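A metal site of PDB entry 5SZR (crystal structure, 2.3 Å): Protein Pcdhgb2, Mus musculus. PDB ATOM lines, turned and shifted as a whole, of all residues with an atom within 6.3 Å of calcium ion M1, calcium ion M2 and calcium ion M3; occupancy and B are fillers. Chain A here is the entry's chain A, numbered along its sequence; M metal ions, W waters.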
ATOM      1  N   GLU A 226      -0.614 -28.294   9.567  1.00  0.00           N
ATOM      2  CA  GLU A 226      -1.194 -27.039   9.137  1.00  0.00           C
ATOM      3  C   GLU A 226      -1.899 -27.174   7.796  1.00  0.00           C
ATOM      4  O   GLU A 226      -1.595 -28.063   7.004  1.00  0.00           O
ATOM      5  CB  GLU A 226      -0.067 -26.001   9.049  1.00  0.00           C
ATOM      6  CG  GLU A 226      -0.404 -24.626   8.610  1.00  0.00           C
ATOM      7  CD  GLU A 226       0.804 -23.726   8.694  1.00  0.00           C
ATOM      8  OE1 GLU A 226       1.894 -24.158   8.258  1.00  0.00           O
ATOM      9  OE2 GLU A 226       0.676 -22.613   9.231  1.00  0.00           O
ATOM     10  N   ASN A 227      -2.862 -26.277   7.559  1.00  0.00           N
ATOM     11  CA  ASN A 227      -3.579 -26.148   6.296  1.00  0.00           C
ATOM     12  C   ASN A 227      -4.443 -27.361   5.985  1.00  0.00           C
ATOM     13  O   ASN A 227      -4.813 -27.603   4.836  1.00  0.00           O
ATOM     14  CB  ASN A 227      -2.617 -25.866   5.136  1.00  0.00           C
ATOM     15  CG  ASN A 227      -1.783 -24.622   5.368  1.00  0.00           C
ATOM     16  OD1 ASN A 227      -2.268 -23.638   5.928  1.00  0.00           O
ATOM     17  ND2 ASN A 227      -0.522 -24.663   4.962  1.00  0.00           N
ATOM     18  N   PHE A 283      -6.030 -25.086  10.250  1.00  0.00           N
ATOM     19  CA  PHE A 283      -5.100 -24.527  11.211  1.00  0.00           C
ATOM     20  C   PHE A 283      -3.949 -23.807  10.496  1.00  0.00           C
ATOM     21  O   PHE A 283      -3.531 -24.202   9.409  1.00  0.00           O
ATOM     22  CB  PHE A 283      -4.551 -25.619  12.130  1.00  0.00           C
ATOM     23  CG  PHE A 283      -5.604 -26.281  12.972  1.00  0.00           C
ATOM     24  CD1 PHE A 283      -5.505 -27.622  13.313  1.00  0.00           C
ATOM     25  CD2 PHE A 283      -6.699 -25.567  13.445  1.00  0.00           C
ATOM     26  CE1 PHE A 283      -6.477 -28.247  14.090  1.00  0.00           C
ATOM     27  CE2 PHE A 283      -7.673 -26.185  14.230  1.00  0.00           C
ATOM     28  CZ  PHE A 283      -7.556 -27.518  14.556  1.00  0.00           C
ATOM     29  N   ASP A 284      -3.443 -22.755  11.132  1.00  0.00           N
ATOM     30  CA  ASP A 284      -2.334 -21.953  10.606  1.00  0.00           C
ATOM     31  C   ASP A 284      -1.257 -21.908  11.682  1.00  0.00           C
ATOM     32  O   ASP A 284      -1.409 -21.216  12.693  1.00  0.00           O
ATOM     33  CB  ASP A 284      -2.820 -20.553  10.225  1.00  0.00           C
ATOM     34  CG  ASP A 284      -1.693 -19.649   9.737  1.00  0.00           C
ATOM     35  OD1 ASP A 284      -0.603 -20.142   9.394  1.00  0.00           O
ATOM     36  OD2 ASP A 284      -1.928 -18.421   9.661  1.00  0.00           O
ATOM     37  N   HIS A 285      -0.177 -22.663  11.459  1.00  0.00           N
ATOM     38  CA  HIS A 285       0.892 -22.765  12.459  1.00  0.00           C
ATOM     39  C   HIS A 285       1.465 -21.402  12.812  1.00  0.00           C
ATOM     40  O   HIS A 285       1.938 -21.193  13.938  1.00  0.00           O
ATOM     41  CB  HIS A 285       1.992 -23.689  11.940  1.00  0.00           C
ATOM     42  CG  HIS A 285       3.222 -23.715  12.796  1.00  0.00           C
ATOM     43  ND1 HIS A 285       3.375 -24.575  13.861  1.00  0.00           N
ATOM     44  CD2 HIS A 285       4.360 -22.980  12.734  1.00  0.00           C
ATOM     45  CE1 HIS A 285       4.558 -24.368  14.428  1.00  0.00           C
ATOM     46  NE2 HIS A 285       5.178 -23.410  13.760  1.00  0.00           N
ATOM     47  N   GLU A 286       1.433 -20.450  11.879  1.00  0.00           N
ATOM     48  CA  GLU A 286       1.997 -19.133  12.133  1.00  0.00           C
ATOM     49  C   GLU A 286       1.119 -18.300  13.083  1.00  0.00           C
ATOM     50  O   GLU A 286       1.644 -17.378  13.716  1.00  0.00           O
ATOM     51  CB  GLU A 286       2.206 -18.399  10.820  1.00  0.00           C
ATOM     52  CG  GLU A 286       3.493 -18.818  10.073  1.00  0.00           C
ATOM     53  CD  GLU A 286       3.447 -20.246   9.534  1.00  0.00           C
ATOM     54  OE1 GLU A 286       2.463 -20.615   8.879  1.00  0.00           O
ATOM     55  OE2 GLU A 286       4.415 -21.000   9.770  1.00  0.00           O
ATOM     56  N   GLN A 287      -0.166 -18.618  13.198  1.00  0.00           N
ATOM     57  CA  GLN A 287      -1.031 -17.929  14.156  1.00  0.00           C
ATOM     58  C   GLN A 287      -1.060 -18.638  15.512  1.00  0.00           C
ATOM     59  O   GLN A 287      -0.948 -17.989  16.554  1.00  0.00           O
ATOM     60  CB  GLN A 287      -2.450 -17.794  13.600  1.00  0.00           C
ATOM     61  CG  GLN A 287      -2.577 -16.753  12.492  1.00  0.00           C
ATOM     62  CD  GLN A 287      -2.163 -15.367  12.929  1.00  0.00           C
ATOM     63  OE1 GLN A 287      -2.548 -14.902  14.005  1.00  0.00           O
ATOM     64  NE2 GLN A 287      -1.356 -14.705  12.113  1.00  0.00           N
ATOM     65  N   GLY A 316       1.173 -28.561  13.268  1.00  0.00           N
ATOM     66  CA  GLY A 316       2.454 -28.821  12.639  1.00  0.00           C
ATOM     67  C   GLY A 316       2.791 -27.781  11.584  1.00  0.00           C
ATOM     68  O   GLY A 316       1.933 -27.335  10.833  1.00  0.00           O
ATOM     69  N   ASP A 317       4.067 -27.407  11.538  1.00  0.00           N
ATOM     70  CA  ASP A 317       4.530 -26.415  10.590  1.00  0.00           C
ATOM     71  C   ASP A 317       4.732 -27.035   9.216  1.00  0.00           C
ATOM     72  O   ASP A 317       5.378 -28.084   9.087  1.00  0.00           O
ATOM     73  CB  ASP A 317       5.833 -25.773  11.080  1.00  0.00           C
ATOM     74  CG  ASP A 317       6.331 -24.686  10.153  1.00  0.00           C
ATOM     75  OD1 ASP A 317       5.483 -23.973   9.565  1.00  0.00           O
ATOM     76  OD2 ASP A 317       7.560 -24.527  10.026  1.00  0.00           O
ATOM     77  N   ARG A 318       4.171 -26.415   8.192  1.00  0.00           N
ATOM     78  CA  ARG A 318       4.467 -26.727   6.805  1.00  0.00           C
ATOM     79  C   ARG A 318       5.191 -25.564   6.149  1.00  0.00           C
ATOM     80  O   ARG A 318       5.209 -24.439   6.675  1.00  0.00           O
ATOM     81  CB  ARG A 318       3.185 -27.053   6.013  1.00  0.00           C
ATOM     82  CG  ARG A 318       2.617 -28.438   6.255  1.00  0.00           C
ATOM     83  CD  ARG A 318       1.529 -28.746   5.245  1.00  0.00           C
ATOM     84  NE  ARG A 318       0.959 -30.074   5.422  1.00  0.00           N
ATOM     85  CZ  ARG A 318       1.515 -31.194   4.947  1.00  0.00           C
ATOM     86  NH1 ARG A 318       0.930 -32.360   5.155  1.00  0.00           N
ATOM     87  NH2 ARG A 318       2.654 -31.126   4.274  1.00  0.00           N
ATOM     88  N   ASN A 319       5.789 -25.828   4.998  1.00  0.00           N
ATOM     89  CA  ASN A 319       6.530 -24.800   4.262  1.00  0.00           C
ATOM     90  C   ASN A 319       5.590 -24.090   3.294  1.00  0.00           C
ATOM     91  O   ASN A 319       5.670 -24.212   2.073  1.00  0.00           O
ATOM     92  CB  ASN A 319       7.723 -25.422   3.530  1.00  0.00           C
ATOM     93  CG  ASN A 319       8.673 -24.361   3.016  1.00  0.00           C
ATOM     94  OD1 ASN A 319       8.897 -23.350   3.675  1.00  0.00           O
ATOM     95  ND2 ASN A 319       9.231 -24.568   1.816  1.00  0.00           N
ATOM     96  N   ASP A 320       4.677 -23.300   3.876  1.00  0.00           N
ATOM     97  CA  ASP A 320       3.730 -22.530   3.086  1.00  0.00           C
ATOM     98  C   ASP A 320       4.107 -21.060   2.973  1.00  0.00           C
ATOM     99  O   ASP A 320       3.281 -20.239   2.555  1.00  0.00           O
ATOM    100  CB  ASP A 320       2.311 -22.688   3.649  1.00  0.00           C
ATOM    101  CG  ASP A 320       2.231 -22.395   5.143  1.00  0.00           C
ATOM    102  OD1 ASP A 320       3.277 -22.324   5.805  1.00  0.00           O
ATOM    103  OD2 ASP A 320       1.092 -22.259   5.651  1.00  0.00           O
ATOM    104  N   ASN A 321       5.336 -20.690   3.328  1.00  0.00           N
ATOM    105  CA  ASN A 321       5.826 -19.330   3.168  1.00  0.00           C
ATOM    106  C   ASN A 321       7.178 -19.381   2.469  1.00  0.00           C
ATOM    107  O   ASN A 321       8.091 -20.063   2.926  1.00  0.00           O
ATOM    108  CB  ASN A 321       5.958 -18.616   4.513  1.00  0.00           C
ATOM    109  CG  ASN A 321       4.615 -18.329   5.143  1.00  0.00           C
ATOM    110  OD1 ASN A 321       4.010 -17.291   4.884  1.00  0.00           O
ATOM    111  ND2 ASN A 321       4.149 -19.245   5.982  1.00  0.00           N
ATOM    112  N   ALA A 322       7.288 -18.668   1.351  1.00  0.00           N
ATOM    113  CA  ALA A 322       8.565 -18.525   0.677  1.00  0.00           C
ATOM    114  C   ALA A 322       9.387 -17.434   1.343  1.00  0.00           C
ATOM    115  O   ALA A 322       8.822 -16.444   1.834  1.00  0.00           O
ATOM    116  CB  ALA A 322       8.371 -18.201  -0.798  1.00  0.00           C
ATOM    117  N   PRO A 323      10.711 -17.578   1.388  1.00  0.00           N
ATOM    118  CA  PRO A 323      11.538 -16.485   1.902  1.00  0.00           C
ATOM    119  C   PRO A 323      11.364 -15.234   1.059  1.00  0.00           C
ATOM    120  O   PRO A 323      11.050 -15.290  -0.128  1.00  0.00           O
ATOM    121  CB  PRO A 323      12.966 -17.042   1.810  1.00  0.00           C
ATOM    122  CG  PRO A 323      12.891 -18.206   0.892  1.00  0.00           C
ATOM    123  CD  PRO A 323      11.499 -18.757   0.992  1.00  0.00           C
ATOM    124  N   ASP A 358      11.794 -15.455   6.760  1.00  0.00           N
ATOM    125  CA  ASP A 358      10.920 -16.561   6.393  1.00  0.00           C
ATOM    126  C   ASP A 358       9.929 -16.782   7.532  1.00  0.00           C
ATOM    127  O   ASP A 358      10.339 -16.984   8.676  1.00  0.00           O
ATOM    128  CB  ASP A 358      11.733 -17.835   6.129  1.00  0.00           C
ATOM    129  CG  ASP A 358      10.943 -18.882   5.366  1.00  0.00           C
ATOM    130  OD1 ASP A 358       9.865 -19.302   5.837  1.00  0.00           O
ATOM    131  OD2 ASP A 358      11.409 -19.302   4.288  1.00  0.00           O
ATOM    132  N   ALA A 359       8.634 -16.738   7.216  1.00  0.00           N
ATOM    133  CA  ALA A 359       7.590 -16.792   8.233  1.00  0.00           C
ATOM    134  C   ALA A 359       7.457 -18.152   8.892  1.00  0.00           C
ATOM    135  O   ALA A 359       6.770 -18.267   9.916  1.00  0.00           O
ATOM    136  CB  ALA A 359       6.249 -16.373   7.640  1.00  0.00           C
ATOM    137  N   ASP A 360       8.072 -19.196   8.340  1.00  0.00           N
ATOM    138  CA  ASP A 360       7.875 -20.544   8.861  1.00  0.00           C
ATOM    139  C   ASP A 360       8.784 -20.814  10.058  1.00  0.00           C
ATOM    140  O   ASP A 360       9.329 -19.867  10.648  1.00  0.00           O
ATOM    141  CB  ASP A 360       8.114 -21.573   7.750  1.00  0.00           C
ATOM    142  CG  ASP A 360       7.126 -21.425   6.611  1.00  0.00           C
ATOM    143  OD1 ASP A 360       5.946 -21.125   6.879  1.00  0.00           O
ATOM    144  OD2 ASP A 360       7.511 -21.616   5.443  1.00  0.00           O
ATOM    145  N   SER A 361       8.946 -22.084  10.422  1.00  0.00           N
ATOM    146  CA  SER A 361       9.757 -22.476  11.563  1.00  0.00           C
ATOM    147  C   SER A 361      10.681 -23.631  11.185  1.00  0.00           C
ATOM    148  O   SER A 361      10.494 -24.275  10.143  1.00  0.00           O
ATOM    149  CB  SER A 361       8.884 -22.883  12.763  1.00  0.00           C
ATOM    150  OG  SER A 361       8.010 -21.829  13.123  1.00  0.00           O
ATOM    151  N   HIS A 363      13.413 -26.109   9.847  1.00  0.00           N
ATOM    152  CA  HIS A 363      14.050 -26.166   8.539  1.00  0.00           C
ATOM    153  C   HIS A 363      13.255 -25.421   7.486  1.00  0.00           C
ATOM    154  O   HIS A 363      13.828 -24.939   6.501  1.00  0.00           O
ATOM    155  CB  HIS A 363      14.259 -27.624   8.113  1.00  0.00           C
ATOM    156  CG  HIS A 363      15.395 -28.300   8.833  1.00  0.00           C
ATOM    157  ND1 HIS A 363      15.264 -28.854  10.077  1.00  0.00           N
ATOM    158  CD2 HIS A 363      16.682 -28.502   8.454  1.00  0.00           C
ATOM    159  CE1 HIS A 363      16.420 -29.379  10.452  1.00  0.00           C
ATOM    160  NE2 HIS A 363      17.298 -29.177   9.488  1.00  0.00           N
ATOM    161  N   ASN A 364      11.939 -25.308   7.663  1.00  0.00           N
ATOM    162  CA  ASN A 364      11.130 -24.565   6.704  1.00  0.00           C
ATOM    163  C   ASN A 364      11.520 -23.087   6.643  1.00  0.00           C
ATOM    164  O   ASN A 364      11.184 -22.402   5.668  1.00  0.00           O
ATOM    165  CB  ASN A 364       9.639 -24.693   7.043  1.00  0.00           C
ATOM    166  CG  ASN A 364       9.115 -26.103   6.828  1.00  0.00           C
ATOM    167  OD1 ASN A 364       9.481 -26.780   5.880  1.00  0.00           O
ATOM    168  ND2 ASN A 364       8.218 -26.538   7.719  1.00  0.00           N
ATOM    169  N   ALA A 365      12.253 -22.584   7.652  1.00  0.00           N
ATOM    170  CA  ALA A 365      12.699 -21.194   7.644  1.00  0.00           C
ATOM    171  C   ALA A 365      14.213 -21.068   7.832  1.00  0.00           C
ATOM    172  O   ALA A 365      14.702 -19.981   8.160  1.00  0.00           O
ATOM    173  CB  ALA A 365      11.972 -20.386   8.728  1.00  0.00           C
ATOM    174  N   LEU A 367      17.461 -20.453   6.259  1.00  0.00           N
ATOM    175  CA  LEU A 367      17.795 -19.886   4.965  1.00  0.00           C
ATOM    176  C   LEU A 367      19.244 -20.165   4.591  1.00  0.00           C
ATOM    177  O   LEU A 367      20.131 -20.189   5.442  1.00  0.00           O
ATOM    178  CB  LEU A 367      17.530 -18.378   4.962  1.00  0.00           C
ATOM    179  CG  LEU A 367      16.079 -18.070   5.323  1.00  0.00           C
ATOM    180  CD1 LEU A 367      15.762 -16.614   5.050  1.00  0.00           C
ATOM    181  CD2 LEU A 367      15.121 -19.007   4.578  1.00  0.00           C
ATOM    182  N   ASP A 411      14.972 -21.787   1.517  1.00  0.00           N
ATOM    183  CA  ASP A 411      14.750 -22.377   2.822  1.00  0.00           C
ATOM    184  C   ASP A 411      15.141 -23.847   2.787  1.00  0.00           C
ATOM    185  O   ASP A 411      15.564 -24.384   1.758  1.00  0.00           O
ATOM    186  CB  ASP A 411      13.317 -22.154   3.304  1.00  0.00           C
ATOM    187  CG  ASP A 411      12.263 -22.759   2.374  1.00  0.00           C
ATOM    188  OD1 ASP A 411      12.531 -23.773   1.696  1.00  0.00           O
ATOM    189  OD2 ASP A 411      11.142 -22.216   2.335  1.00  0.00           O
ATOM    190  N   GLY A 412      15.007 -24.524   3.921  1.00  0.00           N
ATOM    191  CA  GLY A 412      15.412 -25.916   4.012  1.00  0.00           C
ATOM    192  C   GLY A 412      14.248 -26.874   3.909  1.00  0.00           C
ATOM    193  O   GLY A 412      14.377 -28.049   4.275  1.00  0.00           O
ATOM    194  N   GLY A 413      13.111 -26.394   3.417  1.00  0.00           N
ATOM    195  CA  GLY A 413      11.939 -27.218   3.261  1.00  0.00           C
ATOM    196  C   GLY A 413      12.039 -28.173   2.086  1.00  0.00           C
ATOM    197  O   GLY A 413      13.004 -28.176   1.315  1.00  0.00           O
ATOM    198  N   LEU A 417      11.332 -23.599  -1.126  1.00  0.00           N
ATOM    199  CA  LEU A 417      10.930 -22.318  -1.705  1.00  0.00           C
ATOM    200  C   LEU A 417      12.098 -21.340  -1.660  1.00  0.00           C
ATOM    201  O   LEU A 417      12.999 -21.457  -0.819  1.00  0.00           O
ATOM    202  CB  LEU A 417       9.723 -21.741  -0.952  1.00  0.00           C
ATOM    203  CG  LEU A 417       8.492 -22.633  -0.832  1.00  0.00           C
ATOM    204  CD1 LEU A 417       7.427 -21.969   0.023  1.00  0.00           C
ATOM    205  CD2 LEU A 417       7.929 -22.973  -2.209  1.00  0.00           C
HETATM  206 CA    CA M   1       4.215 -22.555   8.001  1.00  0.00          CA
HETATM  207 CA    CA M   2       0.608 -21.030   7.565  1.00  0.00          CA
HETATM  208 CA    CA M   3       9.649 -21.287   4.293  1.00  0.00          CA
HETATM  209  O   HOH W   1       1.042 -18.753   6.414  1.00  0.00           O
HETATM  210  O   HOH W   2      -1.691 -21.172   6.892  1.00  0.00           O
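The backbone NH (N) of Gly 413 sits at hydrogen-bond distance from the side-chain carboxylate (OD1) of Asp 411 (3.2 Å).
The backbone NH (N) of Glu 226 lies close to the backbone carbonyl oxygen (O) of Gly 316, at 3.0 Å.
The side-chain carboxylate of Asp 317 sits at hydrogen-bond distance from the backbone NH of Ser 361.
OD2 of Asp 320 lies close to ND2 of Asn 227 (3.0 Å).
The side-chain carboxylate (OD1) of Asp 320 sits close to the side-chain amide nitrogen (ND2) of Asn 321 (3.2 Å).
The side-chain amide nitrogen (ND2) of Asn 364 is in hydrogen-bond range of the side-chain carboxylate (OD2) of Asp 317 (3.1 Å).
OD1 of Asp 411 lies within hydrogen-bond range of N of Leu 417, at 3.1 Å.
Of the 27 residues printed, 7 come within 4 Å of calcium ion M1.
Along chain A the residues within 4 Å of calcium ion M1 span positions 226 to 360.
Four residues have an atom within 4 Å of calcium ion M2: Glu 226, Asp 284, Glu 286 and Asp 320.
The nearest printed residue that does not touch calcium ion M2 is Asn 227 (4.2 Å).
Of the 27 residues printed, 6 come within 4 Å of calcium ion M3.
Calcium ion M1 is bound by the side-chain carboxylate (OE2) of Glu 286, the side-chain carboxylate (OD1) of Asp 320, the side-chain carboxylate (OD1) of Asp 317, the backbone carbonyl oxygen (O) of Arg 318, the side-chain carboxylate (OD1) of Asp 360, the side-chain carboxylate (OE1) of Glu 286 and the side-chain carboxylate (OE1) of Glu 226.
Calcium ion M1 has seven donor atoms within binding distance.
Calcium ion M2 is bound by OE2 of Glu 226 (2.3 Å), OE1 of Glu 286 (2.3 Å), OD2 of Asp 320 (2.3 Å), OD1 of Asp 284 (2.4 Å), water W2 (2.4 Å) and water W1 (2.6 Å).
Calcium ion M2 has six donor atoms within binding distance.
Calcium ion M3 is bound by the side-chain amide oxygen (OD1) of Asn 319 (2.3 Å), the backbone carbonyl oxygen (O) of Asn 364 (2.3 Å), the backbone carbonyl oxygen (O) of Asn 321 (2.4 Å), the side-chain carboxylate (OD2) of Asp 360 (2.4 Å), the side-chain carboxylate (OD1) of Asp 358 (2.5 Å), the side-chain carboxylate (OD2) of Asp 411 (2.6 Å) and the side-chain carboxylate (OD2) of Asp 358 (2.7 Å).
Calcium ion M3 has seven donor atoms within binding distance.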
